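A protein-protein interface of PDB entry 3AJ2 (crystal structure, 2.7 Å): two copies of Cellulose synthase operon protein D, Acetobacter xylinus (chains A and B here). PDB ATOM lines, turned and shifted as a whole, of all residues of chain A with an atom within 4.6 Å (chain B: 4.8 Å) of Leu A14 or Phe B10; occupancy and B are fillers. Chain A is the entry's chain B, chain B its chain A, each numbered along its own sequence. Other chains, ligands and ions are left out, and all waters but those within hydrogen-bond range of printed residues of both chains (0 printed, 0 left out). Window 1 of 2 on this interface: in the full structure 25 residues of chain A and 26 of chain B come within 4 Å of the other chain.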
ATOM      1  N   PHE A  10       3.532  -0.025   9.825  1.00  0.00           N
ATOM      2  CA  PHE A  10       2.182   0.489   9.944  1.00  0.00           C
ATOM      3  C   PHE A  10       2.064   1.892  10.440  1.00  0.00           C
ATOM      4  O   PHE A  10       0.948   2.419  10.489  1.00  0.00           O
ATOM      5  CB  PHE A  10       1.332  -0.446  10.752  1.00  0.00           C
ATOM      6  CG  PHE A  10       1.267  -1.794  10.143  1.00  0.00           C
ATOM      7  CD1 PHE A  10       0.485  -2.024   9.006  1.00  0.00           C
ATOM      8  CD2 PHE A  10       2.014  -2.836  10.646  1.00  0.00           C
ATOM      9  CE1 PHE A  10       0.450  -3.267   8.417  1.00  0.00           C
ATOM     10  CE2 PHE A  10       1.974  -4.057  10.053  1.00  0.00           C
ATOM     11  CZ  PHE A  10       1.200  -4.281   8.942  1.00  0.00           C
ATOM     12  N   THR A  11       3.178   2.544  10.760  1.00  0.00           N
ATOM     13  CA  THR A  11       3.041   3.849  11.430  1.00  0.00           C
ATOM     14  C   THR A  11       2.180   4.811  10.619  1.00  0.00           C
ATOM     15  O   THR A  11       1.214   5.363  11.132  1.00  0.00           O
ATOM     16  CB  THR A  11       4.370   4.525  11.791  1.00  0.00           C
ATOM     17  OG1 THR A  11       5.166   3.621  12.528  1.00  0.00           O
ATOM     18  CG2 THR A  11       4.104   5.726  12.701  1.00  0.00           C
ATOM     19  N   LEU A  12       2.530   4.982   9.348  1.00  0.00           N
ATOM     20  CA  LEU A  12       1.760   5.863   8.486  1.00  0.00           C
ATOM     21  C   LEU A  12       0.303   5.424   8.368  1.00  0.00           C
ATOM     22  O   LEU A  12      -0.597   6.278   8.441  1.00  0.00           O
ATOM     23  CB  LEU A  12       2.355   5.941   7.092  1.00  0.00           C
ATOM     24  CG  LEU A  12       1.640   6.961   6.235  1.00  0.00           C
ATOM     25  CD1 LEU A  12       2.112   8.317   6.748  1.00  0.00           C
ATOM     26  CD2 LEU A  12       2.058   6.736   4.816  1.00  0.00           C
ATOM     27  N   PHE A  13       0.078   4.113   8.176  1.00  0.00           N
ATOM     28  CA  PHE A  13      -1.278   3.611   8.107  1.00  0.00           C
ATOM     29  C   PHE A  13      -2.070   4.048   9.344  1.00  0.00           C
ATOM     30  O   PHE A  13      -3.152   4.600   9.213  1.00  0.00           O
ATOM     31  CB  PHE A  13      -1.305   2.092   7.919  1.00  0.00           C
ATOM     32  CG  PHE A  13      -2.680   1.493   8.078  1.00  0.00           C
ATOM     33  CD1 PHE A  13      -3.683   1.781   7.155  1.00  0.00           C
ATOM     34  CD2 PHE A  13      -2.971   0.660   9.169  1.00  0.00           C
ATOM     35  CE1 PHE A  13      -4.951   1.263   7.302  1.00  0.00           C
ATOM     36  CE2 PHE A  13      -4.237   0.128   9.327  1.00  0.00           C
ATOM     37  CZ  PHE A  13      -5.239   0.441   8.383  1.00  0.00           C
ATOM     38  N   LEU A  14      -1.497   3.865  10.538  1.00  0.00           N
ATOM     39  CA  LEU A  14      -2.180   4.235  11.760  1.00  0.00           C
ATOM     40  C   LEU A  14      -2.364   5.725  11.891  1.00  0.00           C
ATOM     41  O   LEU A  14      -3.356   6.214  12.467  1.00  0.00           O
ATOM     42  CB  LEU A  14      -1.438   3.714  12.976  1.00  0.00           C
ATOM     43  CG  LEU A  14      -1.824   2.315  13.469  1.00  0.00           C
ATOM     44  CD1 LEU A  14      -3.221   1.881  12.979  1.00  0.00           C
ATOM     45  CD2 LEU A  14      -0.822   1.370  12.997  1.00  0.00           C
ATOM     46  N   GLN A  15      -1.405   6.466  11.355  1.00  0.00           N
ATOM     47  CA  GLN A  15      -1.537   7.913  11.351  1.00  0.00           C
ATOM     48  C   GLN A  15      -2.803   8.279  10.601  1.00  0.00           C
ATOM     49  O   GLN A  15      -3.630   9.053  11.090  1.00  0.00           O
ATOM     50  CB  GLN A  15      -0.319   8.545  10.708  1.00  0.00           C
ATOM     51  CG  GLN A  15       0.791   8.684  11.698  1.00  0.00           C
ATOM     52  CD  GLN A  15       1.982   9.274  11.072  1.00  0.00           C
ATOM     53  OE1 GLN A  15       2.794   8.564  10.457  1.00  0.00           O
ATOM     54  NE2 GLN A  15       2.116  10.596  11.201  1.00  0.00           N
ATOM     55  N   THR A  16      -2.990   7.675   9.437  1.00  0.00           N
ATOM     56  CA  THR A  16      -4.147   8.015   8.675  1.00  0.00           C
ATOM     57  C   THR A  16      -5.409   7.335   9.237  1.00  0.00           C
ATOM     58  O   THR A  16      -6.467   7.989   9.313  1.00  0.00           O
ATOM     59  CB  THR A  16      -3.918   7.835   7.206  1.00  0.00           C
ATOM     60  OG1 THR A  16      -3.440   6.513   7.003  1.00  0.00           O
ATOM     61  CG2 THR A  16      -2.830   8.783   6.764  1.00  0.00           C
ATOM     62  N   LEU A  17      -5.307   6.088   9.703  1.00  0.00           N
ATOM     63  CA  LEU A  17      -6.480   5.463  10.346  1.00  0.00           C
ATOM     64  C   LEU A  17      -7.045   6.267  11.534  1.00  0.00           C
ATOM     65  O   LEU A  17      -8.245   6.553  11.565  1.00  0.00           O
ATOM     66  CB  LEU A  17      -6.216   4.028  10.786  1.00  0.00           C
ATOM     67  CG  LEU A  17      -7.392   3.225  11.366  1.00  0.00           C
ATOM     68  CD1 LEU A  17      -8.482   2.971  10.296  1.00  0.00           C
ATOM     69  CD2 LEU A  17      -6.932   1.896  11.973  1.00  0.00           C
ATOM     70  N   SER A  18      -6.195   6.637  12.497  1.00  0.00           N
ATOM     71  CA  SER A  18      -6.658   7.399  13.651  1.00  0.00           C
ATOM     72  C   SER A  18      -7.378   8.679  13.236  1.00  0.00           C
ATOM     73  O   SER A  18      -8.413   9.051  13.812  1.00  0.00           O
ATOM     74  CB  SER A  18      -5.511   7.727  14.593  1.00  0.00           C
ATOM     75  OG  SER A  18      -4.522   8.495  13.949  1.00  0.00           O
ATOM     76  N   TRP A  69       5.958  -2.371  22.674  1.00  0.00           N
ATOM     77  CA  TRP A  69       5.126  -1.256  23.133  1.00  0.00           C
ATOM     78  C   TRP A  69       5.562  -0.571  24.427  1.00  0.00           C
ATOM     79  O   TRP A  69       4.764   0.186  25.024  1.00  0.00           O
ATOM     80  CB  TRP A  69       3.678  -1.690  23.273  1.00  0.00           C
ATOM     81  CG  TRP A  69       2.929  -1.776  21.974  1.00  0.00           C
ATOM     82  CD1 TRP A  69       3.389  -2.286  20.783  1.00  0.00           C
ATOM     83  CD2 TRP A  69       1.582  -1.389  21.757  1.00  0.00           C
ATOM     84  NE1 TRP A  69       2.405  -2.222  19.838  1.00  0.00           N
ATOM     85  CE2 TRP A  69       1.281  -1.676  20.397  1.00  0.00           C
ATOM     86  CE3 TRP A  69       0.584  -0.838  22.578  1.00  0.00           C
ATOM     87  CZ2 TRP A  69       0.007  -1.435  19.826  1.00  0.00           C
ATOM     88  CZ3 TRP A  69      -0.688  -0.572  22.010  1.00  0.00           C
ATOM     89  CH2 TRP A  69      -0.958  -0.892  20.642  1.00  0.00           C
ATOM     90  N   PRO A  91       3.521   3.605  22.059  1.00  0.00           N
ATOM     91  CA  PRO A  91       3.835   3.930  20.668  1.00  0.00           C
ATOM     92  C   PRO A  91       3.049   5.143  20.183  1.00  0.00           C
ATOM     93  O   PRO A  91       1.847   5.300  20.481  1.00  0.00           O
ATOM     94  CB  PRO A  91       3.385   2.694  19.924  1.00  0.00           C
ATOM     95  CG  PRO A  91       3.666   1.601  20.910  1.00  0.00           C
ATOM     96  CD  PRO A  91       3.217   2.177  22.236  1.00  0.00           C
ATOM     97  N   VAL A  93       1.468   7.414  17.127  1.00  0.00           N
ATOM     98  CA  VAL A  93       1.077   7.287  15.747  1.00  0.00           C
ATOM     99  C   VAL A  93       0.471   8.599  15.338  1.00  0.00           C
ATOM    100  O   VAL A  93      -0.755   8.701  15.208  1.00  0.00           O
ATOM    101  CB  VAL A  93       0.083   6.101  15.488  1.00  0.00           C
ATOM    102  CG1 VAL A  93       0.782   4.720  15.604  1.00  0.00           C
ATOM    103  CG2 VAL A  93      -1.112   6.174  16.394  1.00  0.00           C
ATOM    104  N   LEU A 104      -3.356   5.864  21.213  1.00  0.00           N
ATOM    105  CA  LEU A 104      -3.398   4.423  21.438  1.00  0.00           C
ATOM    106  C   LEU A 104      -3.645   4.116  22.921  1.00  0.00           C
ATOM    107  O   LEU A 104      -3.786   2.945  23.317  1.00  0.00           O
ATOM    108  CB  LEU A 104      -2.093   3.806  20.955  1.00  0.00           C
ATOM    109  CG  LEU A 104      -1.893   2.991  19.661  1.00  0.00           C
ATOM    110  CD1 LEU A 104      -3.125   2.733  18.780  1.00  0.00           C
ATOM    111  CD2 LEU A 104      -0.695   3.516  18.839  1.00  0.00           C
ATOM    112  N   PRO B   8       7.996  -0.123  17.476  1.00  0.00           N
ATOM    113  CA  PRO B   8       6.918  -1.005  17.936  1.00  0.00           C
ATOM    114  C   PRO B   8       6.313  -1.872  16.822  1.00  0.00           C
ATOM    115  O   PRO B   8       6.206  -1.420  15.715  1.00  0.00           O
ATOM    116  CB  PRO B   8       5.867  -0.012  18.459  1.00  0.00           C
ATOM    117  CG  PRO B   8       6.617   1.310  18.576  1.00  0.00           C
ATOM    118  CD  PRO B   8       7.624   1.294  17.536  1.00  0.00           C
ATOM    119  N   ASP B   9       5.934  -3.106  17.132  1.00  0.00           N
ATOM    120  CA  ASP B   9       5.202  -3.943  16.214  1.00  0.00           C
ATOM    121  C   ASP B   9       3.726  -3.565  16.250  1.00  0.00           C
ATOM    122  O   ASP B   9       3.148  -3.455  17.325  1.00  0.00           O
ATOM    123  CB  ASP B   9       5.378  -5.426  16.590  1.00  0.00           C
ATOM    124  CG  ASP B   9       4.443  -6.413  15.732  1.00  0.00           C
ATOM    125  OD1 ASP B   9       4.386  -6.279  14.454  1.00  0.00           O
ATOM    126  OD2 ASP B   9       3.766  -7.327  16.357  1.00  0.00           O
ATOM    127  N   PHE B  10       3.097  -3.383  15.097  1.00  0.00           N
ATOM    128  CA  PHE B  10       1.640  -3.170  15.100  1.00  0.00           C
ATOM    129  C   PHE B  10       0.783  -4.374  14.730  1.00  0.00           C
ATOM    130  O   PHE B  10      -0.435  -4.325  14.899  1.00  0.00           O
ATOM    131  CB  PHE B  10       1.229  -1.895  14.347  1.00  0.00           C
ATOM    132  CG  PHE B  10       1.672  -0.671  15.045  1.00  0.00           C
ATOM    133  CD1 PHE B  10       1.066  -0.282  16.257  1.00  0.00           C
ATOM    134  CD2 PHE B  10       2.753   0.067  14.581  1.00  0.00           C
ATOM    135  CE1 PHE B  10       1.519   0.859  16.972  1.00  0.00           C
ATOM    136  CE2 PHE B  10       3.199   1.185  15.287  1.00  0.00           C
ATOM    137  CZ  PHE B  10       2.588   1.581  16.488  1.00  0.00           C
ATOM    138  N   THR B  11       1.407  -5.473  14.305  1.00  0.00           N
ATOM    139  CA  THR B  11       0.639  -6.620  13.759  1.00  0.00           C
ATOM    140  C   THR B  11      -0.444  -7.113  14.702  1.00  0.00           C
ATOM    141  O   THR B  11      -1.592  -7.189  14.335  1.00  0.00           O
ATOM    142  CB  THR B  11       1.543  -7.833  13.360  1.00  0.00           C
ATOM    143  OG1 THR B  11       2.608  -7.402  12.522  1.00  0.00           O
ATOM    144  CG2 THR B  11       0.743  -8.875  12.619  1.00  0.00           C
ATOM    145  N   LEU B  12      -0.070  -7.432  15.930  1.00  0.00           N
ATOM    146  CA  LEU B  12      -1.019  -7.976  16.882  1.00  0.00           C
ATOM    147  C   LEU B  12      -2.126  -6.976  17.147  1.00  0.00           C
ATOM    148  O   LEU B  12      -3.321  -7.341  17.176  1.00  0.00           O
ATOM    149  CB  LEU B  12      -0.283  -8.274  18.145  1.00  0.00           C
ATOM    150  CG  LEU B  12      -0.729  -9.342  19.114  1.00  0.00           C
ATOM    151  CD1 LEU B  12      -1.180  -8.624  20.359  1.00  0.00           C
ATOM    152  CD2 LEU B  12      -1.790 -10.296  18.548  1.00  0.00           C
ATOM    153  N   PHE B  13      -1.768  -5.704  17.310  1.00  0.00           N
ATOM    154  CA  PHE B  13      -2.815  -4.692  17.351  1.00  0.00           C
ATOM    155  C   PHE B  13      -3.698  -4.763  16.077  1.00  0.00           C
ATOM    156  O   PHE B  13      -4.928  -4.710  16.142  1.00  0.00           O
ATOM    157  CB  PHE B  13      -2.177  -3.327  17.492  1.00  0.00           C
ATOM    158  CG  PHE B  13      -3.143  -2.205  17.461  1.00  0.00           C
ATOM    159  CD1 PHE B  13      -3.926  -1.921  18.564  1.00  0.00           C
ATOM    160  CD2 PHE B  13      -3.252  -1.402  16.324  1.00  0.00           C
ATOM    161  CE1 PHE B  13      -4.836  -0.845  18.537  1.00  0.00           C
ATOM    162  CE2 PHE B  13      -4.151  -0.338  16.264  1.00  0.00           C
ATOM    163  CZ  PHE B  13      -4.949  -0.054  17.379  1.00  0.00           C
ATOM    164  N   LEU B  14      -3.094  -4.879  14.906  1.00  0.00           N
ATOM    165  CA  LEU B  14      -3.933  -4.866  13.749  1.00  0.00           C
ATOM    166  C   LEU B  14      -4.794  -6.113  13.707  1.00  0.00           C
ATOM    167  O   LEU B  14      -5.943  -6.050  13.276  1.00  0.00           O
ATOM    168  CB  LEU B  14      -3.121  -4.669  12.479  1.00  0.00           C
ATOM    169  CG  LEU B  14      -3.109  -3.260  11.833  1.00  0.00           C
ATOM    170  CD1 LEU B  14      -3.859  -2.166  12.614  1.00  0.00           C
ATOM    171  CD2 LEU B  14      -1.732  -2.761  11.416  1.00  0.00           C
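Phe A10 touches its own counterpart, Phe B10.
Phe A10 touches Leu B14, and with the chains exchanged Leu A14 touches Phe B10.
5 positions are printed for both chains.
Leu A12 touches none of the printed residues of chain B.
Leu A14 touches just one residue of chain B: Phe B10 (3.8 Å).
Thr A16 touches none of the printed residues of chain B.
Printed residues of chain B within 4 Å of Val A93: Phe B10 (3.7 Å).
Phe B10 touches six residues of chain A.
Of the printed residues of chain A, Leu B14 touches Phe A10 (3.4 Å).
Among the printed residues, pairs that only touch across the chains: Phe A10 with Phe B10, Phe A10 with Leu B14, Leu A14 with Phe B10, Trp A69 with Phe B10, Trp A69 with Phe B13, Pro A91 with Pro B8, Pro A91 with Phe B10, Val A93 with Phe B10, Leu A104 with Phe B10 and Leu A104 with Phe B13.
OD1 of Asp B9 sits at hydrogen-bond distance from OG1 of Thr B11, at 2.9 Å.
The backbone carbonyl oxygen of Leu A14 lies within hydrogen-bond range of the side-chain hydroxyl of Ser A18 (3.0 Å).
The backbone carbonyl oxygen of Asp B9 sits at hydrogen-bond distance from the indole nitrogen of Trp A69 (2.9 Å).
Hydrophobic or aromatic side chains of chain A that line the printed part of chain B: Phe A10, Leu A14, Trp A69, Pro A91, Val A93 and Leu A104.
Hydrophobic or aromatic side chains of chain B that line the printed part of chain A: Pro B8, Phe B10, Phe B13 and Leu B14.
Among the printed residues, no Asp or Glu carboxylate lies within 4 Å of a Lys or Arg side-chain nitrogen of the other chain.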
